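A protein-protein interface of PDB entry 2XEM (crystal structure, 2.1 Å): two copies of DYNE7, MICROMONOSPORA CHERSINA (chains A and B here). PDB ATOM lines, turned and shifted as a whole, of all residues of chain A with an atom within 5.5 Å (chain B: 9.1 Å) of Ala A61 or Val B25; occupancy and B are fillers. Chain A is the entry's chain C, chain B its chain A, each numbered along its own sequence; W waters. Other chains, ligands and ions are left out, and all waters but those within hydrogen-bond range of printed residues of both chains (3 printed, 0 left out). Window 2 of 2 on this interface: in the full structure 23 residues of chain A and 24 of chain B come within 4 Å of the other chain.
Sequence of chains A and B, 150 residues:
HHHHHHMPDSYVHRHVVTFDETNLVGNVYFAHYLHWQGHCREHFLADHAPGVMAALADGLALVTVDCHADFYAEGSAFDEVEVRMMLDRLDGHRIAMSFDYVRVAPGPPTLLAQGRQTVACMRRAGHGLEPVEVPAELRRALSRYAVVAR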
ATOM      1  N   LEU A  56     -28.888 -16.418  -4.922  1.00  0.00           N
ATOM      2  CA  LEU A  56     -27.660 -17.221  -4.814  1.00  0.00           C
ATOM      3  C   LEU A  56     -27.113 -17.410  -3.373  1.00  0.00           C
ATOM      4  O   LEU A  56     -26.147 -18.169  -3.172  1.00  0.00           O
ATOM      5  CB  LEU A  56     -26.555 -16.684  -5.723  1.00  0.00           C
ATOM      6  CG  LEU A  56     -26.862 -16.614  -7.222  1.00  0.00           C
ATOM      7  CD1 LEU A  56     -25.785 -15.869  -7.924  1.00  0.00           C
ATOM      8  CD2 LEU A  56     -27.015 -17.998  -7.840  1.00  0.00           C
ATOM      9  N   GLY A  59     -30.253 -20.478  -1.846  1.00  0.00           N
ATOM     10  CA  GLY A  59     -30.432 -21.812  -2.412  1.00  0.00           C
ATOM     11  C   GLY A  59     -30.322 -21.955  -3.920  1.00  0.00           C
ATOM     12  O   GLY A  59     -30.128 -23.071  -4.401  1.00  0.00           O
ATOM     13  N   LEU A  60     -30.479 -20.853  -4.686  1.00  0.00           N
ATOM     14  CA  LEU A  60     -30.214 -20.876  -6.134  1.00  0.00           C
ATOM     15  C   LEU A  60     -28.713 -21.028  -6.394  1.00  0.00           C
ATOM     16  O   LEU A  60     -27.893 -20.428  -5.688  1.00  0.00           O
ATOM     17  CB  LEU A  60     -30.774 -19.631  -6.842  1.00  0.00           C
ATOM     18  CG  LEU A  60     -30.653 -19.590  -8.378  1.00  0.00           C
ATOM     19  CD1 LEU A  60     -31.596 -20.630  -9.042  1.00  0.00           C
ATOM     20  CD2 LEU A  60     -30.900 -18.157  -8.918  1.00  0.00           C
ATOM     21  N   ALA A  61     -28.357 -21.862  -7.376  1.00  0.00           N
ATOM     22  CA  ALA A  61     -26.965 -22.069  -7.782  1.00  0.00           C
ATOM     23  C   ALA A  61     -26.839 -22.014  -9.278  1.00  0.00           C
ATOM     24  O   ALA A  61     -27.695 -22.549  -9.993  1.00  0.00           O
ATOM     25  CB  ALA A  61     -26.466 -23.412  -7.277  1.00  0.00           C
ATOM     26  N   LEU A  62     -25.759 -21.397  -9.758  1.00  0.00           N
ATOM     27  CA  LEU A  62     -25.420 -21.454 -11.181  1.00  0.00           C
ATOM     28  C   LEU A  62     -24.375 -22.554 -11.369  1.00  0.00           C
ATOM     29  O   LEU A  62     -23.242 -22.458 -10.853  1.00  0.00           O
ATOM     30  CB  LEU A  62     -24.906 -20.102 -11.706  1.00  0.00           C
ATOM     31  CG  LEU A  62     -25.815 -18.890 -11.628  1.00  0.00           C
ATOM     32  CD1 LEU A  62     -25.091 -17.661 -12.135  1.00  0.00           C
ATOM     33  CD2 LEU A  62     -27.090 -19.102 -12.415  1.00  0.00           C
ATOM     34  N   VAL A  63     -24.770 -23.611 -12.072  1.00  0.00           N
ATOM     35  CA  VAL A  63     -23.917 -24.782 -12.227  1.00  0.00           C
ATOM     36  C   VAL A  63     -23.352 -24.818 -13.637  1.00  0.00           C
ATOM     37  O   VAL A  63     -24.119 -24.771 -14.584  1.00  0.00           O
ATOM     38  CB  VAL A  63     -24.690 -26.070 -11.843  1.00  0.00           C
ATOM     39  CG1 VAL A  63     -23.853 -27.325 -12.099  1.00  0.00           C
ATOM     40  CG2 VAL A  63     -25.134 -26.014 -10.374  1.00  0.00           C
ATOM     41  N   ALA A 120     -26.296 -23.804 -15.913  1.00  0.00           N
ATOM     42  CA  ALA A 120     -27.662 -24.232 -15.587  1.00  0.00           C
ATOM     43  C   ALA A 120     -28.073 -23.625 -14.259  1.00  0.00           C
ATOM     44  O   ALA A 120     -27.238 -23.534 -13.364  1.00  0.00           O
ATOM     45  CB  ALA A 120     -27.725 -25.753 -15.503  1.00  0.00           C
ATOM     46  N   CYS A 121     -29.322 -23.150 -14.141  1.00  0.00           N
ATOM     47  CA  CYS A 121     -29.855 -22.769 -12.839  1.00  0.00           C
ATOM     48  C   CYS A 121     -30.335 -23.990 -12.091  1.00  0.00           C
ATOM     49  O   CYS A 121     -31.105 -24.782 -12.622  1.00  0.00           O
ATOM     50  CB  CYS A 121     -30.960 -21.735 -12.963  1.00  0.00           C
ATOM     51  SG  CYS A 121     -30.386 -20.135 -13.536  1.00  0.00           S
ATOM     52  N   MET A 122     -29.867 -24.140 -10.862  1.00  0.00           N
ATOM     53  CA  MET A 122     -30.162 -25.302 -10.056  1.00  0.00           C
ATOM     54  C   MET A 122     -30.488 -24.919  -8.613  1.00  0.00           C
ATOM     55  O   MET A 122     -30.152 -23.824  -8.152  1.00  0.00           O
ATOM     56  CB  MET A 122     -29.009 -26.329 -10.149  1.00  0.00           C
ATOM     57  CG  MET A 122     -28.836 -26.881 -11.576  1.00  0.00           C
ATOM     58  SD  MET A 122     -27.855 -28.364 -11.719  1.00  0.00           S
ATOM     59  CE  MET A 122     -29.056 -29.522 -11.763  1.00  0.00           C
ATOM     60  N   ARG A 123     -31.232 -25.807  -7.948  1.00  0.00           N
ATOM     61  CA  ARG A 123     -31.523 -25.756  -6.527  1.00  0.00           C
ATOM     62  C   ARG A 123     -31.114 -27.091  -5.936  1.00  0.00           C
ATOM     63  O   ARG A 123     -31.197 -28.125  -6.613  1.00  0.00           O
ATOM     64  CB  ARG A 123     -33.018 -25.493  -6.266  1.00  0.00           C
ATOM     65  CG  ARG A 123     -33.416 -24.058  -6.560  1.00  0.00           C
ATOM     66  CD  ARG A 123     -34.498 -23.566  -5.621  1.00  0.00           C
ATOM     67  NE  ARG A 123     -33.971 -22.574  -4.683  1.00  0.00           N
ATOM     68  CZ  ARG A 123     -34.047 -21.260  -4.857  1.00  0.00           C
ATOM     69  NH1 ARG A 123     -34.654 -20.759  -5.925  1.00  0.00           N
ATOM     70  NH2 ARG A 123     -33.529 -20.437  -3.960  1.00  0.00           N
ATOM     71  N   ARG A 124     -30.659 -27.070  -4.676  1.00  0.00           N
ATOM     72  CA  ARG A 124     -30.245 -28.279  -3.982  1.00  0.00           C
ATOM     73  C   ARG A 124     -31.447 -28.879  -3.264  1.00  0.00           C
ATOM     74  O   ARG A 124     -32.105 -28.192  -2.481  1.00  0.00           O
ATOM     75  CB  ARG A 124     -29.103 -27.959  -3.020  1.00  0.00           C
ATOM     76  CG  ARG A 124     -28.271 -29.151  -2.638  1.00  0.00           C
ATOM     77  CD  ARG A 124     -26.846 -28.705  -2.487  1.00  0.00           C
ATOM     78  NE  ARG A 124     -25.948 -29.844  -2.576  1.00  0.00           N
ATOM     79  CZ  ARG A 124     -24.803 -29.842  -3.232  1.00  0.00           C
ATOM     80  NH1 ARG A 124     -24.394 -28.751  -3.861  1.00  0.00           N
ATOM     81  NH2 ARG A 124     -24.034 -30.920  -3.235  1.00  0.00           N
ATOM     82  N   LEU A 129     -28.439 -31.605  -6.563  1.00  0.00           N
ATOM     83  CA  LEU A 129     -28.795 -30.455  -7.402  1.00  0.00           C
ATOM     84  C   LEU A 129     -29.831 -30.830  -8.459  1.00  0.00           C
ATOM     85  O   LEU A 129     -29.652 -31.831  -9.151  1.00  0.00           O
ATOM     86  CB  LEU A 129     -27.547 -29.842  -8.058  1.00  0.00           C
ATOM     87  CG  LEU A 129     -26.562 -29.126  -7.128  1.00  0.00           C
ATOM     88  CD1 LEU A 129     -25.274 -28.855  -7.843  1.00  0.00           C
ATOM     89  CD2 LEU A 129     -27.134 -27.818  -6.594  1.00  0.00           C
ATOM     90  N   THR B  22     -13.380 -26.005  -3.442  1.00  0.00           N
ATOM     91  CA  THR B  22     -14.836 -25.963  -3.369  1.00  0.00           C
ATOM     92  C   THR B  22     -15.285 -24.498  -3.430  1.00  0.00           C
ATOM     93  O   THR B  22     -14.460 -23.595  -3.640  1.00  0.00           O
ATOM     94  CB  THR B  22     -15.351 -26.747  -2.148  1.00  0.00           C
ATOM     95  OG1 THR B  22     -14.991 -26.068  -0.946  1.00  0.00           O
ATOM     96  CG2 THR B  22     -14.866 -28.214  -2.141  1.00  0.00           C
ATOM     97  N   ASN B  23     -16.595 -24.270  -3.310  1.00  0.00           N
ATOM     98  CA  ASN B  23     -17.172 -22.930  -3.254  1.00  0.00           C
ATOM     99  C   ASN B  23     -18.442 -23.015  -2.446  1.00  0.00           C
ATOM    100  O   ASN B  23     -18.822 -24.115  -2.031  1.00  0.00           O
ATOM    101  CB  ASN B  23     -17.375 -22.368  -4.669  1.00  0.00           C
ATOM    102  CG  ASN B  23     -18.487 -23.038  -5.422  1.00  0.00           C
ATOM    103  OD1 ASN B  23     -19.585 -22.504  -5.480  1.00  0.00           O
ATOM    104  ND2 ASN B  23     -18.264 -24.243  -5.917  1.00  0.00           N
ATOM    105  N   LEU B  24     -19.097 -21.879  -2.193  1.00  0.00           N
ATOM    106  CA  LEU B  24     -20.285 -21.849  -1.327  1.00  0.00           C
ATOM    107  C   LEU B  24     -21.439 -22.761  -1.770  1.00  0.00           C
ATOM    108  O   LEU B  24     -22.215 -23.197  -0.928  1.00  0.00           O
ATOM    109  CB  LEU B  24     -20.753 -20.431  -1.025  1.00  0.00           C
ATOM    110  CG  LEU B  24     -21.363 -19.657  -2.168  1.00  0.00           C
ATOM    111  CD1 LEU B  24     -22.888 -19.828  -2.207  1.00  0.00           C
ATOM    112  CD2 LEU B  24     -21.057 -18.198  -2.019  1.00  0.00           C
ATOM    113  N   VAL B  25     -21.554 -23.050  -3.086  1.00  0.00           N
ATOM    114  CA  VAL B  25     -22.551 -24.015  -3.607  1.00  0.00           C
ATOM    115  C   VAL B  25     -22.329 -25.434  -2.992  1.00  0.00           C
ATOM    116  O   VAL B  25     -23.288 -26.181  -2.808  1.00  0.00           O
ATOM    117  CB  VAL B  25     -22.647 -23.994  -5.158  1.00  0.00           C
ATOM    118  CG1 VAL B  25     -23.662 -25.016  -5.681  1.00  0.00           C
ATOM    119  CG2 VAL B  25     -23.011 -22.591  -5.649  1.00  0.00           C
ATOM    120  N   GLY B  26     -21.081 -25.725  -2.607  1.00  0.00           N
ATOM    121  CA  GLY B  26     -20.697 -26.954  -1.922  1.00  0.00           C
ATOM    122  C   GLY B  26     -19.987 -27.952  -2.811  1.00  0.00           C
ATOM    123  O   GLY B  26     -19.528 -28.983  -2.321  1.00  0.00           O
ATOM    124  N   ASN B  27     -19.895 -27.658  -4.112  1.00  0.00           N
ATOM    125  CA  ASN B  27     -19.186 -28.468  -5.104  1.00  0.00           C
ATOM    126  C   ASN B  27     -17.809 -27.906  -5.473  1.00  0.00           C
ATOM    127  O   ASN B  27     -17.433 -26.834  -5.003  1.00  0.00           O
ATOM    128  CB  ASN B  27     -20.050 -28.695  -6.369  1.00  0.00           C
ATOM    129  CG  ASN B  27     -20.641 -27.454  -6.981  1.00  0.00           C
ATOM    130  OD1 ASN B  27     -20.056 -26.364  -6.983  1.00  0.00           O
ATOM    131  ND2 ASN B  27     -21.835 -27.588  -7.534  1.00  0.00           N
ATOM    132  N   VAL B  28     -17.055 -28.646  -6.301  1.00  0.00           N
ATOM    133  CA  VAL B  28     -15.797 -28.161  -6.860  1.00  0.00           C
ATOM    134  C   VAL B  28     -16.116 -27.037  -7.858  1.00  0.00           C
ATOM    135  O   VAL B  28     -16.903 -27.247  -8.768  1.00  0.00           O
ATOM    136  CB  VAL B  28     -14.961 -29.307  -7.514  1.00  0.00           C
ATOM    137  CG1 VAL B  28     -13.671 -28.766  -8.152  1.00  0.00           C
ATOM    138  CG2 VAL B  28     -14.639 -30.389  -6.496  1.00  0.00           C
ATOM    139  N   TYR B  29     -15.541 -25.840  -7.650  1.00  0.00           N
ATOM    140  CA  TYR B  29     -15.669 -24.743  -8.588  1.00  0.00           C
ATOM    141  C   TYR B  29     -15.151 -25.147  -9.977  1.00  0.00           C
ATOM    142  O   TYR B  29     -14.068 -25.727 -10.077  1.00  0.00           O
ATOM    143  CB  TYR B  29     -14.944 -23.486  -8.061  1.00  0.00           C
ATOM    144  CG  TYR B  29     -15.274 -22.251  -8.865  1.00  0.00           C
ATOM    145  CD1 TYR B  29     -14.396 -21.771  -9.837  1.00  0.00           C
ATOM    146  CD2 TYR B  29     -16.510 -21.619  -8.732  1.00  0.00           C
ATOM    147  CE1 TYR B  29     -14.720 -20.662 -10.616  1.00  0.00           C
ATOM    148  CE2 TYR B  29     -16.827 -20.487  -9.475  1.00  0.00           C
ATOM    149  CZ  TYR B  29     -15.935 -20.016 -10.421  1.00  0.00           C
ATOM    150  OH  TYR B  29     -16.265 -18.891 -11.145  1.00  0.00           O
ATOM    151  N   PHE B  30     -15.926 -24.838 -11.044  1.00  0.00           N
ATOM    152  CA  PHE B  30     -15.692 -25.448 -12.377  1.00  0.00           C
ATOM    153  C   PHE B  30     -14.261 -25.284 -12.906  1.00  0.00           C
ATOM    154  O   PHE B  30     -13.738 -26.197 -13.520  1.00  0.00           O
ATOM    155  CB  PHE B  30     -16.727 -24.935 -13.414  1.00  0.00           C
ATOM    156  CG  PHE B  30     -16.402 -23.553 -13.956  1.00  0.00           C
ATOM    157  CD1 PHE B  30     -15.709 -23.403 -15.153  1.00  0.00           C
ATOM    158  CD2 PHE B  30     -16.759 -22.406 -13.252  1.00  0.00           C
ATOM    159  CE1 PHE B  30     -15.378 -22.130 -15.633  1.00  0.00           C
ATOM    160  CE2 PHE B  30     -16.419 -21.136 -13.727  1.00  0.00           C
ATOM    161  CZ  PHE B  30     -15.732 -21.012 -14.919  1.00  0.00           C
ATOM    162  N   GLU B  74     -21.489 -33.494  -9.691  1.00  0.00           N
ATOM    163  CA  GLU B  74     -20.664 -32.662  -8.817  1.00  0.00           C
ATOM    164  C   GLU B  74     -19.589 -33.408  -8.063  1.00  0.00           C
ATOM    165  O   GLU B  74     -19.788 -34.564  -7.657  1.00  0.00           O
ATOM    166  CB  GLU B  74     -21.514 -31.748  -7.904  1.00  0.00           C
ATOM    167  CG  GLU B  74     -22.368 -32.447  -6.883  1.00  0.00           C
ATOM    168  CD  GLU B  74     -23.337 -31.551  -6.131  1.00  0.00           C
ATOM    169  OE1 GLU B  74     -23.043 -30.352  -5.909  1.00  0.00           O
ATOM    170  OE2 GLU B  74     -24.383 -32.083  -5.703  1.00  0.00           O
ATOM    171  N   GLY B  75     -18.438 -32.752  -7.949  1.00  0.00           N
ATOM    172  CA  GLY B  75     -17.351 -33.192  -7.088  1.00  0.00           C
ATOM    173  C   GLY B  75     -17.500 -32.514  -5.740  1.00  0.00           C
ATOM    174  O   GLY B  75     -18.067 -31.425  -5.660  1.00  0.00           O
ATOM    175  N   SER B  76     -16.963 -33.121  -4.689  1.00  0.00           N
ATOM    176  CA  SER B  76     -17.043 -32.585  -3.321  1.00  0.00           C
ATOM    177  C   SER B  76     -15.654 -32.645  -2.679  1.00  0.00           C
ATOM    178  O   SER B  76     -14.794 -33.400  -3.160  1.00  0.00           O
ATOM    179  CB  SER B  76     -18.023 -33.416  -2.496  1.00  0.00           C
ATOM    180  OG  SER B  76     -19.335 -33.407  -3.037  1.00  0.00           O
HETATM  181  O   HOH W   1     -21.307 -31.338  -3.063  1.00  0.00           O
HETATM  182  O   HOH W   2     -25.882 -33.139  -7.390  1.00  0.00           O
HETATM  183  O   HOH W   3     -21.928 -24.843  -8.956  1.00  0.00           O
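No position is printed for both chains.
Of the 6 pairs that touch across the chains among the printed residues, none has its exchanged pair printed and touching as well.
Hydrophobic or aromatic side chains of chain A that line the printed part of chain B: Ala A61 and Leu A129.
Along chain A the printed residues that touch a printed residue of chain B span positions 56 to 129.
ND2 of Asn B23 lies within hydrogen-bond range of O of Asn B27, 2.9 Å away.
The backbone carbonyl oxygen (O) of Met A122 lies within hydrogen-bond range of the backbone NH (N) of Ala A61 (2.8 Å).
The side-chain amide nitrogen of Asn B27 lies within hydrogen-bond range of the side-chain carboxylate of Glu B74 (3.4 Å).
The side-chain amide oxygen of Asn B23 lies within hydrogen-bond range of the backbone NH of Val B25 (3.1 Å).
The guanidinium group of Arg A124 lies within salt-bridge range of the side-chain carboxylate of Glu B74.
The guanidinium group (NH1) of Arg A124 sits at hydrogen-bond distance from the backbone carbonyl oxygen (O) of Val B25.
Water W2 lies within hydrogen-bond range of OE2 of Glu B74 (2.5 Å) and N of Leu A129 (3.1 Å).
Water W1 lies within hydrogen-bond range of the guanidinium group of Arg A124, the side-chain hydroxyl of Ser B76, the backbone carbonyl oxygen of Gly B26 and the side-chain carboxylate of Glu B74.
Water W3 lies within hydrogen-bond range of the side-chain amide nitrogen (ND2) of Asn B27 and the backbone carbonyl oxygen (O) of Leu A62.
Val B25 touches two residues of chain A.
No residue of chain B comes within 4 Å of Leu A60.
Printed residues of chain A within 4 Å of Glu B74: Arg A124 (2.8 Å) and Leu A129 (3.3 Å).
Of the printed residues of chain B, Arg A124 touches Val B25 and Glu B74.
Arg A123 touches none of the printed residues of chain B.
The nearest residue of chain B that does not touch Ala A61 is Asn B27 (6.2 Å).
The nearest printed residue of chain B that does not touch Arg A124 is Gly B26 (4.5 Å).
Among the printed residues, pairs that only touch across the chains: Leu A56 with Leu B24, Ala A61 with Val B25, Leu A129 with Asn B27 and Leu A129 with Glu B74.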
